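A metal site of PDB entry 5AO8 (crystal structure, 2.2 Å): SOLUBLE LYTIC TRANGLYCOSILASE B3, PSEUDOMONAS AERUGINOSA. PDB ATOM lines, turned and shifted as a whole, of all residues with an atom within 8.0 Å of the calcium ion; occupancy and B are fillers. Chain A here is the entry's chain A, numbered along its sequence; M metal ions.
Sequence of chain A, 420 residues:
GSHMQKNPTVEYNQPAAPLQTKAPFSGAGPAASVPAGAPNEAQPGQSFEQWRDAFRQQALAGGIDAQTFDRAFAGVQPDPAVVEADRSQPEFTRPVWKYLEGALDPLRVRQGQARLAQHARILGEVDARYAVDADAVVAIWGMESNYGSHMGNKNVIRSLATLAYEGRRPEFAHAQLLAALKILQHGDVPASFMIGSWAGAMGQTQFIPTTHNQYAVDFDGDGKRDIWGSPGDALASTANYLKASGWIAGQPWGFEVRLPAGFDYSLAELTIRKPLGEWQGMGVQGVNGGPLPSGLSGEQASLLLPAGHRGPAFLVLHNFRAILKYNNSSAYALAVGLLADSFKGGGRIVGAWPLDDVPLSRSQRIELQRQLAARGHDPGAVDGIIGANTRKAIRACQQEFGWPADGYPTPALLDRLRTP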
ATOM      1  N   ASP A 188      12.720  21.997   6.131  1.00  0.00           N
ATOM      2  CA  ASP A 188      12.145  20.648   6.076  1.00  0.00           C
ATOM      3  C   ASP A 188      11.541  20.273   4.744  1.00  0.00           C
ATOM      4  O   ASP A 188      11.466  19.089   4.389  1.00  0.00           O
ATOM      5  CB  ASP A 188      11.091  20.492   7.149  1.00  0.00           C
ATOM      6  CG  ASP A 188      11.711  20.462   8.572  1.00  0.00           C
ATOM      7  OD1 ASP A 188      12.865  19.966   8.782  1.00  0.00           O
ATOM      8  OD2 ASP A 188      10.987  20.933   9.495  1.00  0.00           O
ATOM      9  N   VAL A 217       9.687  14.255  13.366  1.00  0.00           N
ATOM     10  CA  VAL A 217      10.983  13.610  13.555  1.00  0.00           C
ATOM     11  C   VAL A 217      11.713  13.393  12.242  1.00  0.00           C
ATOM     12  O   VAL A 217      11.112  13.106  11.223  1.00  0.00           O
ATOM     13  CB  VAL A 217      10.817  12.223  14.235  1.00  0.00           C
ATOM     14  CG1 VAL A 217      12.129  11.483  14.326  1.00  0.00           C
ATOM     15  CG2 VAL A 217      10.261  12.396  15.620  1.00  0.00           C
ATOM     16  N   ASP A 218      13.017  13.521  12.304  1.00  0.00           N
ATOM     17  CA  ASP A 218      13.908  13.220  11.208  1.00  0.00           C
ATOM     18  C   ASP A 218      14.468  11.844  11.480  1.00  0.00           C
ATOM     19  O   ASP A 218      15.389  11.719  12.277  1.00  0.00           O
ATOM     20  CB  ASP A 218      15.019  14.270  11.138  1.00  0.00           C
ATOM     21  CG  ASP A 218      16.080  13.936  10.106  1.00  0.00           C
ATOM     22  OD1 ASP A 218      15.744  13.305   9.097  1.00  0.00           O
ATOM     23  OD2 ASP A 218      17.248  14.345  10.257  1.00  0.00           O
ATOM     24  N   PHE A 219      13.916  10.819  10.845  1.00  0.00           N
ATOM     25  CA  PHE A 219      14.263   9.411  11.091  1.00  0.00           C
ATOM     26  C   PHE A 219      15.645   9.017  10.469  1.00  0.00           C
ATOM     27  O   PHE A 219      16.525   8.562  11.162  1.00  0.00           O
ATOM     28  CB  PHE A 219      13.160   8.524  10.515  1.00  0.00           C
ATOM     29  CG  PHE A 219      13.367   7.064  10.742  1.00  0.00           C
ATOM     30  CD1 PHE A 219      13.228   6.510  12.001  1.00  0.00           C
ATOM     31  CD2 PHE A 219      13.686   6.250   9.685  1.00  0.00           C
ATOM     32  CE1 PHE A 219      13.442   5.169  12.204  1.00  0.00           C
ATOM     33  CE2 PHE A 219      13.890   4.909   9.866  1.00  0.00           C
ATOM     34  CZ  PHE A 219      13.768   4.358  11.113  1.00  0.00           C
ATOM     35  N   ASP A 220      15.831   9.200   9.165  1.00  0.00           N
ATOM     36  CA  ASP A 220      17.187   9.323   8.605  1.00  0.00           C
ATOM     37  C   ASP A 220      17.498  10.646   9.256  1.00  0.00           C
ATOM     38  O   ASP A 220      16.559  11.235   9.714  1.00  0.00           O
ATOM     39  CB  ASP A 220      17.196   9.261   7.096  1.00  0.00           C
ATOM     40  CG  ASP A 220      16.476  10.445   6.417  1.00  0.00           C
ATOM     41  OD1 ASP A 220      15.358  10.859   6.799  1.00  0.00           O
ATOM     42  OD2 ASP A 220      17.041  10.951   5.410  1.00  0.00           O
ATOM     43  N   GLY A 221      18.690  11.179   9.384  1.00  0.00           N
ATOM     44  CA  GLY A 221      19.770  11.086   8.475  1.00  0.00           C
ATOM     45  C   GLY A 221      20.017  12.565   8.206  1.00  0.00           C
ATOM     46  O   GLY A 221      20.961  13.152   8.689  1.00  0.00           O
ATOM     47  N   ASP A 222      19.084  13.196   7.501  1.00  0.00           N
ATOM     48  CA  ASP A 222      19.485  14.239   6.574  1.00  0.00           C
ATOM     49  C   ASP A 222      19.219  15.640   7.031  1.00  0.00           C
ATOM     50  O   ASP A 222      19.351  16.555   6.225  1.00  0.00           O
ATOM     51  CB  ASP A 222      18.784  14.003   5.260  1.00  0.00           C
ATOM     52  CG  ASP A 222      17.238  14.177   5.342  1.00  0.00           C
ATOM     53  OD1 ASP A 222      16.653  14.320   6.465  1.00  0.00           O
ATOM     54  OD2 ASP A 222      16.608  14.154   4.264  1.00  0.00           O
ATOM     55  N   GLY A 223      18.795  15.813   8.283  1.00  0.00           N
ATOM     56  CA  GLY A 223      18.476  17.123   8.793  1.00  0.00           C
ATOM     57  C   GLY A 223      17.048  17.608   8.559  1.00  0.00           C
ATOM     58  O   GLY A 223      16.680  18.616   9.105  1.00  0.00           O
ATOM     59  N   LYS A 224      16.262  16.906   7.740  1.00  0.00           N
ATOM     60  CA  LYS A 224      14.913  17.362   7.413  1.00  0.00           C
ATOM     61  C   LYS A 224      13.860  16.526   8.031  1.00  0.00           C
ATOM     62  O   LYS A 224      13.890  15.302   7.899  1.00  0.00           O
ATOM     63  CB  LYS A 224      14.671  17.372   5.910  1.00  0.00           C
ATOM     64  CG  LYS A 224      15.691  18.202   5.127  1.00  0.00           C
ATOM     65  CD  LYS A 224      15.235  18.563   3.751  1.00  0.00           C
ATOM     66  CE  LYS A 224      14.719  17.405   2.924  1.00  0.00           C
ATOM     67  NZ  LYS A 224      13.914  17.921   1.726  1.00  0.00           N
ATOM     68  N   ARG A 225      12.888  17.183   8.651  1.00  0.00           N
ATOM     69  CA  ARG A 225      11.691  16.464   9.114  1.00  0.00           C
ATOM     70  C   ARG A 225      10.671  16.476   8.007  1.00  0.00           C
ATOM     71  O   ARG A 225       9.765  17.305   7.985  1.00  0.00           O
ATOM     72  CB  ARG A 225      11.190  17.094  10.366  1.00  0.00           C
ATOM     73  CG  ARG A 225      12.275  17.180  11.362  1.00  0.00           C
ATOM     74  CD  ARG A 225      11.739  17.552  12.704  1.00  0.00           C
ATOM     75  NE  ARG A 225      11.481  18.972  12.819  1.00  0.00           N
ATOM     76  CZ  ARG A 225      10.881  19.538  13.862  1.00  0.00           C
ATOM     77  NH1 ARG A 225      10.437  18.804  14.917  1.00  0.00           N
ATOM     78  NH2 ARG A 225      10.706  20.845  13.842  1.00  0.00           N
ATOM     79  N   ASP A 226      10.831  15.575   7.061  1.00  0.00           N
ATOM     80  CA  ASP A 226      10.074  15.657   5.831  1.00  0.00           C
ATOM     81  C   ASP A 226       8.854  14.754   5.860  1.00  0.00           C
ATOM     82  O   ASP A 226       8.897  13.609   5.417  1.00  0.00           O
ATOM     83  CB  ASP A 226      10.998  15.335   4.646  1.00  0.00           C
ATOM     84  CG  ASP A 226      10.261  15.163   3.310  1.00  0.00           C
ATOM     85  OD1 ASP A 226       9.126  15.697   3.084  1.00  0.00           O
ATOM     86  OD2 ASP A 226      10.860  14.451   2.470  1.00  0.00           O
ATOM     87  N   ILE A 227       7.747  15.253   6.378  1.00  0.00           N
ATOM     88  CA  ILE A 227       6.547  14.417   6.452  1.00  0.00           C
ATOM     89  C   ILE A 227       5.816  14.366   5.107  1.00  0.00           C
ATOM     90  O   ILE A 227       4.743  13.811   5.017  1.00  0.00           O
ATOM     91  CB  ILE A 227       5.580  14.931   7.547  1.00  0.00           C
ATOM     92  CG1 ILE A 227       5.207  16.404   7.301  1.00  0.00           C
ATOM     93  CG2 ILE A 227       6.226  14.742   8.893  1.00  0.00           C
ATOM     94  CD1 ILE A 227       4.191  16.898   8.267  1.00  0.00           C
ATOM     95  N   SER A 230       8.983  11.556   2.833  1.00  0.00           N
ATOM     96  CA  SER A 230       9.765  10.531   3.510  1.00  0.00           C
ATOM     97  C   SER A 230       8.932   9.720   4.446  1.00  0.00           C
ATOM     98  O   SER A 230       8.527  10.196   5.503  1.00  0.00           O
ATOM     99  CB  SER A 230      10.934  11.129   4.292  1.00  0.00           C
ATOM    100  OG  SER A 230      11.316  10.166   5.272  1.00  0.00           O
ATOM    101  N   GLY A 232       9.802   7.205   6.361  1.00  0.00           N
ATOM    102  CA  GLY A 232      10.539   7.149   7.610  1.00  0.00           C
ATOM    103  C   GLY A 232      10.212   8.264   8.577  1.00  0.00           C
ATOM    104  O   GLY A 232       9.695   8.001   9.688  1.00  0.00           O
ATOM    105  N   ASP A 233      10.443   9.499   8.142  1.00  0.00           N
ATOM    106  CA  ASP A 233      10.087  10.675   8.924  1.00  0.00           C
ATOM    107  C   ASP A 233       8.616  10.655   9.311  1.00  0.00           C
ATOM    108  O   ASP A 233       8.251  10.976  10.412  1.00  0.00           O
ATOM    109  CB  ASP A 233      10.343  11.934   8.147  1.00  0.00           C
ATOM    110  CG  ASP A 233      11.839  12.181   7.850  1.00  0.00           C
ATOM    111  OD1 ASP A 233      12.706  11.368   8.259  1.00  0.00           O
ATOM    112  OD2 ASP A 233      12.128  13.212   7.215  1.00  0.00           O
ATOM    113  N   ALA A 234       7.792  10.320   8.345  1.00  0.00           N
ATOM    114  CA  ALA A 234       6.336  10.355   8.559  1.00  0.00           C
ATOM    115  C   ALA A 234       5.878   9.326   9.623  1.00  0.00           C
ATOM    116  O   ALA A 234       5.161   9.656  10.536  1.00  0.00           O
ATOM    117  CB  ALA A 234       5.602  10.154   7.218  1.00  0.00           C
HETATM  118 CA    CA M   1      14.586  13.209   7.044  1.00  0.00          CA
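OD2 of Asp 218 lies within hydrogen-bond range of N of Gly 223, at 2.9 Å.
The backbone NH (N) of Asp 226 sits close to the side-chain carboxylate (OD2) of Asp 233 (2.7 Å).
OD1 of Asp 233 lies close to N of Phe 219 (2.9 Å).
The backbone NH of Asp 233 lies within hydrogen-bond range of the side-chain hydroxyl of Ser 230 (3.1 Å).
The calcium ion is bound by OD1 of Asp 218 (2.4 Å).
O of Lys 224 binds the calcium ion (2.4 Å).
The calcium ion is bound by the side-chain carboxylate (OD1) of Asp 222 (2.4 Å).
The side-chain carboxylate (OD2) of Asp 233 binds the calcium ion.
OD1 of Asp 220 binds the calcium ion, 2.5 Å away.
The calcium ion is bound by OD1 of Asp 233 (2.9 Å).
Five residues have an atom within 4 Å of the calcium ion: Asp 218, Asp 220, Asp 222, Lys 224 and Asp 233.
Along chain A the residues within 4 Å of the calcium ion span positions 218 to 233.
The nearest printed residue that does not touch the calcium ion is Asp 226 (4.4 Å).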
